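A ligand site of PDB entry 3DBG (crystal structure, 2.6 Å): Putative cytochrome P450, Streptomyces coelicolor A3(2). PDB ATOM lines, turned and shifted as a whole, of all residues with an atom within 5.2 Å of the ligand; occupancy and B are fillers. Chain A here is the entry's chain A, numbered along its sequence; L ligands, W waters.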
ATOM      1  N   PHE A 123      -7.008  -7.907   5.771  1.00  0.00           N
ATOM      2  CA  PHE A 123      -8.005  -7.514   4.780  1.00  0.00           C
ATOM      3  C   PHE A 123      -7.449  -6.645   3.633  1.00  0.00           C
ATOM      4  O   PHE A 123      -8.197  -6.246   2.757  1.00  0.00           O
ATOM      5  CB  PHE A 123      -9.148  -6.763   5.484  1.00  0.00           C
ATOM      6  CG  PHE A 123      -9.893  -7.584   6.492  1.00  0.00           C
ATOM      7  CD1 PHE A 123      -9.643  -7.455   7.859  1.00  0.00           C
ATOM      8  CD2 PHE A 123     -10.876  -8.496   6.074  1.00  0.00           C
ATOM      9  CE1 PHE A 123     -10.368  -8.209   8.825  1.00  0.00           C
ATOM     10  CE2 PHE A 123     -11.604  -9.257   7.032  1.00  0.00           C
ATOM     11  CZ  PHE A 123     -11.352  -9.111   8.399  1.00  0.00           C
ATOM     12  N   ALA A 166     -16.260 -16.545   5.451  1.00  0.00           N
ATOM     13  CA  ALA A 166     -15.633 -15.724   6.473  1.00  0.00           C
ATOM     14  C   ALA A 166     -14.729 -16.526   7.400  1.00  0.00           C
ATOM     15  O   ALA A 166     -13.544 -16.236   7.550  1.00  0.00           O
ATOM     16  CB  ALA A 166     -16.714 -15.011   7.301  1.00  0.00           C
ATOM     17  N   LEU A 170     -10.614 -16.317   7.112  1.00  0.00           N
ATOM     18  CA  LEU A 170     -10.104 -15.570   8.268  1.00  0.00           C
ATOM     19  C   LEU A 170      -9.590 -16.491   9.379  1.00  0.00           C
ATOM     20  O   LEU A 170      -8.942 -16.025  10.321  1.00  0.00           O
ATOM     21  CB  LEU A 170     -11.238 -14.686   8.781  1.00  0.00           C
ATOM     22  CG  LEU A 170     -11.791 -13.724   7.730  1.00  0.00           C
ATOM     23  CD1 LEU A 170     -12.930 -12.976   8.333  1.00  0.00           C
ATOM     24  CD2 LEU A 170     -10.710 -12.765   7.266  1.00  0.00           C
ATOM     25  N   ALA A 270     -16.708 -10.501  17.392  1.00  0.00           N
ATOM     26  CA  ALA A 270     -17.266  -9.219  17.010  1.00  0.00           C
ATOM     27  C   ALA A 270     -17.076  -8.914  15.517  1.00  0.00           C
ATOM     28  O   ALA A 270     -17.820  -8.133  14.926  1.00  0.00           O
ATOM     29  CB  ALA A 270     -16.620  -8.091  17.876  1.00  0.00           C
ATOM     30  N   ILE A 271     -16.091  -9.514  14.898  1.00  0.00           N
ATOM     31  CA  ILE A 271     -15.870  -9.233  13.489  1.00  0.00           C
ATOM     32  C   ILE A 271     -16.636 -10.195  12.607  1.00  0.00           C
ATOM     33  O   ILE A 271     -17.207  -9.811  11.591  1.00  0.00           O
ATOM     34  CB  ILE A 271     -14.365  -9.320  13.175  1.00  0.00           C
ATOM     35  CG1 ILE A 271     -13.656  -8.176  13.903  1.00  0.00           C
ATOM     36  CG2 ILE A 271     -14.136  -9.294  11.668  1.00  0.00           C
ATOM     37  CD1 ILE A 271     -12.127  -8.221  13.872  1.00  0.00           C
ATOM     38  N   LEU A 272     -16.652 -11.450  12.999  1.00  0.00           N
ATOM     39  CA  LEU A 272     -17.286 -12.477  12.210  1.00  0.00           C
ATOM     40  C   LEU A 272     -18.804 -12.409  12.272  1.00  0.00           C
ATOM     41  O   LEU A 272     -19.488 -12.714  11.301  1.00  0.00           O
ATOM     42  CB  LEU A 272     -16.813 -13.849  12.713  1.00  0.00           C
ATOM     43  CG  LEU A 272     -16.783 -15.015  11.719  1.00  0.00           C
ATOM     44  CD1 LEU A 272     -15.445 -15.014  10.945  1.00  0.00           C
ATOM     45  CD2 LEU A 272     -16.951 -16.326  12.477  1.00  0.00           C
ATOM     46  N   GLY A 275     -20.272  -9.241   9.892  1.00  0.00           N
ATOM     47  CA  GLY A 275     -19.811  -9.565   8.564  1.00  0.00           C
ATOM     48  C   GLY A 275     -20.532 -10.722   7.914  1.00  0.00           C
ATOM     49  O   GLY A 275     -20.741 -10.718   6.704  1.00  0.00           O
ATOM     50  N   SER A 276     -20.917 -11.713   8.691  1.00  0.00           N
ATOM     51  CA  SER A 276     -21.619 -12.842   8.104  1.00  0.00           C
ATOM     52  C   SER A 276     -23.038 -12.491   7.754  1.00  0.00           C
ATOM     53  O   SER A 276     -23.462 -12.701   6.623  1.00  0.00           O
ATOM     54  CB  SER A 276     -21.585 -14.009   9.072  1.00  0.00           C
ATOM     55  OG  SER A 276     -20.246 -14.441   9.110  1.00  0.00           O
ATOM     56  N   THR A 278     -24.170  -9.708   7.222  1.00  0.00           N
ATOM     57  CA  THR A 278     -24.094  -8.644   6.226  1.00  0.00           C
ATOM     58  C   THR A 278     -23.876  -9.184   4.808  1.00  0.00           C
ATOM     59  O   THR A 278     -24.593  -8.784   3.882  1.00  0.00           O
ATOM     60  CB  THR A 278     -22.945  -7.673   6.570  1.00  0.00           C
ATOM     61  OG1 THR A 278     -23.065  -7.246   7.935  1.00  0.00           O
ATOM     62  CG2 THR A 278     -23.015  -6.428   5.711  1.00  0.00           C
ATOM     63  N   ILE A 279     -22.903 -10.083   4.633  1.00  0.00           N
ATOM     64  CA  ILE A 279     -22.627 -10.667   3.330  1.00  0.00           C
ATOM     65  C   ILE A 279     -23.781 -11.587   2.937  1.00  0.00           C
ATOM     66  O   ILE A 279     -24.113 -11.710   1.775  1.00  0.00           O
ATOM     67  CB  ILE A 279     -21.254 -11.449   3.342  1.00  0.00           C
ATOM     68  CG1 ILE A 279     -20.487 -11.240   2.044  1.00  0.00           C
ATOM     69  CG2 ILE A 279     -21.481 -12.926   3.416  1.00  0.00           C
ATOM     70  CD1 ILE A 279     -19.598 -10.027   2.001  1.00  0.00           C
ATOM     71  N   THR A 282     -26.631  -9.703   1.651  1.00  0.00           N
ATOM     72  CA  THR A 282     -26.259  -9.217   0.323  1.00  0.00           C
ATOM     73  C   THR A 282     -26.418 -10.331  -0.721  1.00  0.00           C
ATOM     74  O   THR A 282     -26.825 -10.101  -1.849  1.00  0.00           O
ATOM     75  CB  THR A 282     -24.822  -8.678   0.344  1.00  0.00           C
ATOM     76  OG1 THR A 282     -24.777  -7.510   1.168  1.00  0.00           O
ATOM     77  CG2 THR A 282     -24.363  -8.270  -1.035  1.00  0.00           C
ATOM     78  N   ALA A 337     -27.480  -4.053   2.630  1.00  0.00           N
ATOM     79  CA  ALA A 337     -27.681  -4.707   3.908  1.00  0.00           C
ATOM     80  C   ALA A 337     -27.654  -3.645   4.985  1.00  0.00           C
ATOM     81  O   ALA A 337     -28.594  -3.562   5.779  1.00  0.00           O
ATOM     82  CB  ALA A 337     -26.590  -5.748   4.146  1.00  0.00           C
ATOM     83  N   VAL A 338     -26.598  -2.835   5.040  1.00  0.00           N
ATOM     84  CA  VAL A 338     -26.605  -1.765   6.032  1.00  0.00           C
ATOM     85  C   VAL A 338     -27.310  -0.524   5.435  1.00  0.00           C
ATOM     86  O   VAL A 338     -26.818   0.106   4.515  1.00  0.00           O
ATOM     87  CB  VAL A 338     -25.127  -1.460   6.560  1.00  0.00           C
ATOM     88  CG1 VAL A 338     -24.098  -1.673   5.484  1.00  0.00           C
ATOM     89  CG2 VAL A 338     -25.051  -0.037   7.095  1.00  0.00           C
ATOM     90  N   LEU A 341     -26.699   4.313   9.521  1.00  0.00           N
ATOM     91  CA  LEU A 341     -25.400   4.453  10.156  1.00  0.00           C
ATOM     92  C   LEU A 341     -25.473   5.596  11.169  1.00  0.00           C
ATOM     93  O   LEU A 341     -26.190   6.571  10.940  1.00  0.00           O
ATOM     94  CB  LEU A 341     -24.322   4.734   9.096  1.00  0.00           C
ATOM     95  CG  LEU A 341     -23.947   3.605   8.110  1.00  0.00           C
ATOM     96  CD1 LEU A 341     -22.815   4.048   7.209  1.00  0.00           C
ATOM     97  CD2 LEU A 341     -23.543   2.368   8.886  1.00  0.00           C
ATOM     98  N   THR A 342     -24.759   5.465  12.297  1.00  0.00           N
ATOM     99  CA  THR A 342     -24.818   6.485  13.344  1.00  0.00           C
ATOM    100  C   THR A 342     -23.459   7.015  13.682  1.00  0.00           C
ATOM    101  O   THR A 342     -22.443   6.326  13.505  1.00  0.00           O
ATOM    102  CB  THR A 342     -25.397   5.945  14.668  1.00  0.00           C
ATOM    103  OG1 THR A 342     -26.245   4.839  14.399  1.00  0.00           O
ATOM    104  CG2 THR A 342     -26.204   7.027  15.386  1.00  0.00           C
ATOM    105  N   ARG A 343     -23.442   8.241  14.177  1.00  0.00           N
ATOM    106  CA  ARG A 343     -22.220   8.901  14.570  1.00  0.00           C
ATOM    107  C   ARG A 343     -22.466   9.769  15.781  1.00  0.00           C
ATOM    108  O   ARG A 343     -23.602  10.184  16.009  1.00  0.00           O
ATOM    109  CB  ARG A 343     -21.679   9.790  13.439  1.00  0.00           C
ATOM    110  CG  ARG A 343     -21.216   9.032  12.187  1.00  0.00           C
ATOM    111  CD  ARG A 343     -20.115   7.997  12.456  1.00  0.00           C
ATOM    112  NE  ARG A 343     -19.582   7.445  11.195  1.00  0.00           N
ATOM    113  CZ  ARG A 343     -18.338   7.029  11.020  1.00  0.00           C
ATOM    114  NH1 ARG A 343     -17.465   7.084  12.033  1.00  0.00           N
ATOM    115  NH2 ARG A 343     -17.952   6.557   9.829  1.00  0.00           N
ATOM    116  N   TYR A 364     -27.854   8.760   9.559  1.00  0.00           N
ATOM    117  CA  TYR A 364     -28.013   8.896   8.119  1.00  0.00           C
ATOM    118  C   TYR A 364     -28.272   7.529   7.490  1.00  0.00           C
ATOM    119  O   TYR A 364     -27.933   6.473   8.051  1.00  0.00           O
ATOM    120  CB  TYR A 364     -26.788   9.610   7.476  1.00  0.00           C
ATOM    121  CG  TYR A 364     -25.451   8.884   7.460  1.00  0.00           C
ATOM    122  CD1 TYR A 364     -25.059   8.128   6.335  1.00  0.00           C
ATOM    123  CD2 TYR A 364     -24.547   8.996   8.537  1.00  0.00           C
ATOM    124  CE1 TYR A 364     -23.822   7.507   6.275  1.00  0.00           C
ATOM    125  CE2 TYR A 364     -23.302   8.357   8.488  1.00  0.00           C
ATOM    126  CZ  TYR A 364     -22.957   7.618   7.341  1.00  0.00           C
ATOM    127  OH  TYR A 364     -21.747   6.982   7.238  1.00  0.00           O
ATOM    128  N   PRO A 402     -21.233   1.804  -0.033  1.00  0.00           N
ATOM    129  CA  PRO A 402     -21.711   0.687   0.792  1.00  0.00           C
ATOM    130  C   PRO A 402     -20.856   0.536   2.028  1.00  0.00           C
ATOM    131  O   PRO A 402     -21.357   0.221   3.093  1.00  0.00           O
ATOM    132  CB  PRO A 402     -21.632  -0.495  -0.143  1.00  0.00           C
ATOM    133  CG  PRO A 402     -21.810   0.124  -1.483  1.00  0.00           C
ATOM    134  CD  PRO A 402     -20.994   1.361  -1.416  1.00  0.00           C
ATOM    135  N   PHE A 403     -19.550   0.741   1.850  1.00  0.00           N
ATOM    136  CA  PHE A 403     -18.607   0.756   2.960  1.00  0.00           C
ATOM    137  C   PHE A 403     -18.242   2.270   3.158  1.00  0.00           C
ATOM    138  O   PHE A 403     -18.341   3.044   2.206  1.00  0.00           O
ATOM    139  CB  PHE A 403     -17.380  -0.083   2.588  1.00  0.00           C
ATOM    140  CG  PHE A 403     -17.704  -1.343   1.786  1.00  0.00           C
ATOM    141  CD1 PHE A 403     -17.917  -1.285   0.409  1.00  0.00           C
ATOM    142  CD2 PHE A 403     -17.741  -2.600   2.393  1.00  0.00           C
ATOM    143  CE1 PHE A 403     -18.177  -2.477  -0.350  1.00  0.00           C
ATOM    144  CE2 PHE A 403     -17.994  -3.809   1.646  1.00  0.00           C
ATOM    145  CZ  PHE A 403     -18.204  -3.746   0.276  1.00  0.00           C
ATOM    146  N   SER A 404     -17.844   2.730   4.346  1.00  0.00           N
ATOM    147  CA  SER A 404     -17.580   4.192   4.490  1.00  0.00           C
ATOM    148  C   SER A 404     -16.092   4.575   4.233  1.00  0.00           C
ATOM    149  O   SER A 404     -15.272   3.688   3.999  1.00  0.00           O
ATOM    150  CB  SER A 404     -18.047   4.634   5.874  1.00  0.00           C
ATOM    151  OG  SER A 404     -19.388   4.201   6.065  1.00  0.00           O
ATOM    152  N   LYS A 407     -11.667   5.913   9.072  1.00  0.00           N
ATOM    153  CA  LYS A 407     -11.301   4.604   9.644  1.00  0.00           C
ATOM    154  C   LYS A 407     -12.535   3.747   9.969  1.00  0.00           C
ATOM    155  O   LYS A 407     -12.501   2.552   9.693  1.00  0.00           O
ATOM    156  CB  LYS A 407     -10.416   4.746  10.898  1.00  0.00           C
ATOM    157  CG  LYS A 407      -9.068   3.941  10.795  1.00  0.00           C
ATOM    158  CD  LYS A 407      -9.116   2.467  11.296  1.00  0.00           C
ATOM    159  CE  LYS A 407      -7.875   1.659  10.845  1.00  0.00           C
ATOM    160  NZ  LYS A 407      -7.707   0.369  11.587  1.00  0.00           N
ATOM    161  N   ARG A 408     -13.607   4.294  10.568  1.00  0.00           N
ATOM    162  CA  ARG A 408     -14.787   3.431  10.724  1.00  0.00           C
ATOM    163  C   ARG A 408     -15.333   3.153   9.312  1.00  0.00           C
ATOM    164  O   ARG A 408     -16.321   3.737   8.885  1.00  0.00           O
ATOM    165  CB  ARG A 408     -15.895   4.101  11.555  1.00  0.00           C
ATOM    166  CG  ARG A 408     -15.802   4.041  13.104  1.00  0.00           C
ATOM    167  CD  ARG A 408     -17.203   4.358  13.742  1.00  0.00           C
ATOM    168  NE  ARG A 408     -17.176   5.107  15.025  1.00  0.00           N
ATOM    169  CZ  ARG A 408     -18.246   5.494  15.716  1.00  0.00           C
ATOM    170  NH1 ARG A 408     -19.483   5.224  15.285  1.00  0.00           N
ATOM    171  NH2 ARG A 408     -18.104   6.170  16.845  1.00  0.00           N
ATOM    172  N   LYS A 409     -14.653   2.267   8.595  1.00  0.00           N
ATOM    173  CA  LYS A 409     -14.926   1.885   7.216  1.00  0.00           C
ATOM    174  C   LYS A 409     -15.054   0.391   7.166  1.00  0.00           C
ATOM    175  O   LYS A 409     -14.979  -0.225   8.203  1.00  0.00           O
ATOM    176  CB  LYS A 409     -13.773   2.385   6.369  1.00  0.00           C
ATOM    177  CG  LYS A 409     -13.463   1.696   5.054  1.00  0.00           C
ATOM    178  CD  LYS A 409     -12.428   2.528   4.261  1.00  0.00           C
ATOM    179  CE  LYS A 409     -12.406   2.203   2.763  1.00  0.00           C
ATOM    180  NZ  LYS A 409     -11.447   3.062   1.976  1.00  0.00           N
ATOM    181  N   CYS A 410     -15.238  -0.234   6.013  1.00  0.00           N
ATOM    182  CA  CYS A 410     -15.294  -1.674   6.105  1.00  0.00           C
ATOM    183  C   CYS A 410     -13.998  -2.310   5.636  1.00  0.00           C
ATOM    184  O   CYS A 410     -13.672  -2.245   4.442  1.00  0.00           O
ATOM    185  CB  CYS A 410     -16.433  -2.207   5.292  1.00  0.00           C
ATOM    186  SG  CYS A 410     -16.530  -3.991   5.587  1.00  0.00           S
ATOM    187  N   PRO A 411     -13.251  -2.952   6.550  1.00  0.00           N
ATOM    188  CA  PRO A 411     -11.972  -3.615   6.262  1.00  0.00           C
ATOM    189  C   PRO A 411     -12.080  -4.661   5.176  1.00  0.00           C
ATOM    190  O   PRO A 411     -11.108  -4.931   4.471  1.00  0.00           O
ATOM    191  CB  PRO A 411     -11.565  -4.218   7.600  1.00  0.00           C
ATOM    192  CG  PRO A 411     -12.283  -3.371   8.604  1.00  0.00           C
ATOM    193  CD  PRO A 411     -13.610  -3.181   7.967  1.00  0.00           C
ATOM    194  N   SER A 412     -13.271  -5.235   5.044  1.00  0.00           N
ATOM    195  CA  SER A 412     -13.526  -6.300   4.087  1.00  0.00           C
ATOM    196  C   SER A 412     -14.131  -5.816   2.789  1.00  0.00           C
ATOM    197  O   SER A 412     -14.825  -6.565   2.111  1.00  0.00           O
ATOM    198  CB  SER A 412     -14.450  -7.338   4.697  1.00  0.00           C
ATOM    199  OG  SER A 412     -14.064  -7.559   6.032  1.00  0.00           O
ATOM    200  N   PHE A 415     -12.251  -7.976   0.366  1.00  0.00           N
ATOM    201  CA  PHE A 415     -12.581  -9.355   0.714  1.00  0.00           C
ATOM    202  C   PHE A 415     -14.045  -9.649   0.418  1.00  0.00           C
ATOM    203  O   PHE A 415     -14.405 -10.773   0.083  1.00  0.00           O
ATOM    204  CB  PHE A 415     -12.271  -9.574   2.189  1.00  0.00           C
ATOM    205  CG  PHE A 415     -12.699 -10.893   2.733  1.00  0.00           C
ATOM    206  CD1 PHE A 415     -13.846 -11.000   3.532  1.00  0.00           C
ATOM    207  CD2 PHE A 415     -11.939 -12.054   2.463  1.00  0.00           C
ATOM    208  CE1 PHE A 415     -14.240 -12.236   4.080  1.00  0.00           C
ATOM    209  CE2 PHE A 415     -12.331 -13.308   2.998  1.00  0.00           C
ATOM    210  CZ  PHE A 415     -13.487 -13.401   3.816  1.00  0.00           C
ATOM    211  N   SER A 416     -14.913  -8.643   0.542  1.00  0.00           N
ATOM    212  CA  SER A 416     -16.321  -8.827   0.261  1.00  0.00           C
ATOM    213  C   SER A 416     -16.575  -8.953  -1.211  1.00  0.00           C
ATOM    214  O   SER A 416     -17.027  -9.993  -1.666  1.00  0.00           O
ATOM    215  CB  SER A 416     -17.125  -7.658   0.798  1.00  0.00           C
ATOM    216  OG  SER A 416     -17.170  -7.770   2.200  1.00  0.00           O
ATOM    217  N   GLN A 419     -15.413 -12.282  -2.829  1.00  0.00           N
ATOM    218  CA  GLN A 419     -16.163 -13.521  -2.685  1.00  0.00           C
ATOM    219  C   GLN A 419     -17.545 -13.417  -3.317  1.00  0.00           C
ATOM    220  O   GLN A 419     -18.072 -14.397  -3.842  1.00  0.00           O
ATOM    221  CB  GLN A 419     -16.298 -13.892  -1.202  1.00  0.00           C
ATOM    222  CG  GLN A 419     -17.325 -13.105  -0.408  1.00  0.00           C
ATOM    223  CD  GLN A 419     -16.998 -13.082   1.063  1.00  0.00           C
ATOM    224  OE1 GLN A 419     -16.039 -12.440   1.470  1.00  0.00           O
ATOM    225  NE2 GLN A 419     -17.791 -13.787   1.872  1.00  0.00           N
ATOM    226  N   LEU A 420     -18.136 -12.221  -3.274  1.00  0.00           N
ATOM    227  CA  LEU A 420     -19.455 -12.026  -3.880  1.00  0.00           C
ATOM    228  C   LEU A 420     -19.366 -12.197  -5.398  1.00  0.00           C
ATOM    229  O   LEU A 420     -20.234 -12.834  -6.008  1.00  0.00           O
ATOM    230  CB  LEU A 420     -20.011 -10.610  -3.547  1.00  0.00           C
ATOM    231  CG  LEU A 420     -20.284 -10.201  -2.076  1.00  0.00           C
ATOM    232  CD1 LEU A 420     -20.836  -8.814  -2.073  1.00  0.00           C
ATOM    233  CD2 LEU A 420     -21.254 -11.144  -1.404  1.00  0.00           C
HETATM  234  C1  LIG L   1     -17.852  -2.046   9.474  1.00  0.00           C
HETATM  235  C2  LIG L   1     -20.465  -2.470   5.320  1.00  0.00           C
HETATM  236  C3  LIG L   1     -18.893  -7.170   4.872  1.00  0.00           C
HETATM  237  C4  LIG L   1     -16.278  -6.705   9.047  1.00  0.00           C
HETATM  238  C5  LIG L   1     -18.696  -1.717   8.399  1.00  0.00           C
HETATM  239  C6  LIG L   1     -19.368  -0.426   8.205  1.00  0.00           C
HETATM  240  C7  LIG L   1     -20.117  -0.526   7.002  1.00  0.00           C
HETATM  241  C8  LIG L   1     -19.916  -1.891   6.483  1.00  0.00           C
HETATM  242  C9  LIG L   1     -21.022   0.541   6.344  1.00  0.00           C
HETATM  243  C10 LIG L   1     -19.181   0.772   9.230  1.00  0.00           C
HETATM  244  C11 LIG L   1     -19.429   2.188   8.810  1.00  0.00           C
HETATM  245  C12 LIG L   1     -19.620   3.096  10.012  1.00  0.00           C
HETATM  246  O1  LIG L   1     -18.915   4.152   9.993  1.00  0.00           O
HETATM  247  O2  LIG L   1     -20.436   2.787  10.898  1.00  0.00           O
HETATM  248  C13 LIG L   1     -20.280  -3.792   4.801  1.00  0.00           C
HETATM  249  C14 LIG L   1     -20.879  -4.326   3.582  1.00  0.00           C
HETATM  250  C15 LIG L   1     -20.424  -5.652   3.451  1.00  0.00           C
HETATM  251  C16 LIG L   1     -19.575  -5.939   4.584  1.00  0.00           C
HETATM  252  C17 LIG L   1     -21.796  -3.564   2.625  1.00  0.00           C
HETATM  253  C18 LIG L   1     -20.752  -6.642   2.335  1.00  0.00           C
HETATM  254  C19 LIG L   1     -22.093  -7.309   2.505  1.00  0.00           C
HETATM  255  C20 LIG L   1     -18.046  -7.470   5.976  1.00  0.00           C
HETATM  256  C21 LIG L   1     -17.384  -8.776   6.197  1.00  0.00           C
HETATM  257  C22 LIG L   1     -16.639  -8.647   7.368  1.00  0.00           C
HETATM  258  C23 LIG L   1     -16.842  -7.288   7.879  1.00  0.00           C
HETATM  259  C24 LIG L   1     -17.511 -10.014   5.259  1.00  0.00           C
HETATM  260  C25 LIG L   1     -15.742  -9.713   8.052  1.00  0.00           C
HETATM  261  C26 LIG L   1     -16.480 -10.860   8.731  1.00  0.00           C
HETATM  262  C27 LIG L   1     -16.461  -5.402   9.553  1.00  0.00           C
HETATM  263  C28 LIG L   1     -15.853  -4.846  10.765  1.00  0.00           C
HETATM  264  C29 LIG L   1     -16.301  -3.526  10.898  1.00  0.00           C
HETATM  265  C30 LIG L   1     -17.167  -3.267   9.740  1.00  0.00           C
HETATM  266  C31 LIG L   1     -14.913  -5.599  11.720  1.00  0.00           C
HETATM  267  C32 LIG L   1     -15.924  -2.524  12.028  1.00  0.00           C
HETATM  268  C33 LIG L   1     -14.904  -1.411  11.587  1.00  0.00           C
HETATM  269  C34 LIG L   1     -14.593  -0.425  12.699  1.00  0.00           C
HETATM  270  O3  LIG L   1     -14.687  -0.752  13.904  1.00  0.00           O
HETATM  271  O4  LIG L   1     -14.251   0.706  12.298  1.00  0.00           O
HETATM  272  N1  LIG L   1     -19.032  -2.581   7.360  1.00  0.00           N
HETATM  273  N2  LIG L   1     -19.467  -4.808   5.414  1.00  0.00           N
HETATM  274  N3  LIG L   1     -17.713  -6.565   7.011  1.00  0.00           N
HETATM  275  N4  LIG L   1     -17.255  -4.411   8.939  1.00  0.00           N
HETATM  276 FE1  LIG L   1     -18.229  -4.521   7.098  1.00  0.00          FE
HETATM  277  O   HOH W   1     -20.005  -2.736  12.009  1.00  0.00           O
HETATM  278  O   HOH W   2     -20.638  -4.074   9.215  1.00  0.00           O
HETATM  279  O   HOH W   3     -12.720   0.160   9.951  1.00  0.00           O
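The side-chain sulfur of Cys 410 is bound to an iron atom (FE1) of the ligand, 2.3 Å away. O of Arg 408 lies close to O1 of the ligand. The guanidinium group (NH2) of Arg 343 is in salt-bridge range of an oxygen (O1) of the ligand, 2.6 Å away.
NH2 of Arg 343 sits at hydrogen-bond distance from O of Arg 408, at 3.4 Å. N of Leu 341 is in hydrogen-bond range of O of Tyr 364, at 2.9 Å. OG of Ser 416 sits at hydrogen-bond distance from O of Ser 412 (2.6 Å). O of Leu 272 lies within hydrogen-bond range of OG of Ser 276 (2.9 Å). SG of Cys 410 lies close to N of Ser 412, 3.5 Å away. The side-chain hydroxyl (OG1) of Thr 282 sits at hydrogen-bond distance from the backbone carbonyl oxygen (O) of Thr 278 (3.0 Å).
Ile 271 touches the ligand. CA of Leu 272 touches C26 of the ligand, 3.9 Å away. Gly 275 touches the ligand (CA to C21, 3.5 Å). Thr 278 touches the ligand (O to C19, 3.2 Å). Ile 279 touches the ligand (CA to C19, 3.5 Å). Thr 282 touches the ligand (OG1 to C19, 3.0 Å). CG1 of Val 338 touches C2 of the ligand, 3.7 Å away. Leu 341 touches the ligand (CD2 to O2, 3.7 Å). O of Pro 402 touches C9 of the ligand, at 3.3 Å. Phe 403 touches the ligand (CE2 to C14, 3.5 Å). Ser 404 touches the ligand. Lys 407 touches the ligand. Lys 409 touches the ligand (O to C33, 3.6 Å). Pro 411 touches the ligand (CD to C27, 3.9 Å). Ser 412 touches the ligand (OG to C22, 3.1 Å). Ser 416 touches the ligand. Hydrophobic or aromatic side chains that line the ligand: Ile 271, Ile 279, Val 338, Leu 341, Phe 403 and Pro 411. Of the 30 residues printed, 19 come within 4 Å of the ligand.
Water W3 lies within hydrogen-bond range of O of Lys 407 (2.4 Å), O4 of the ligand (2.9 Å) and O of Lys 409 (2.9 Å).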
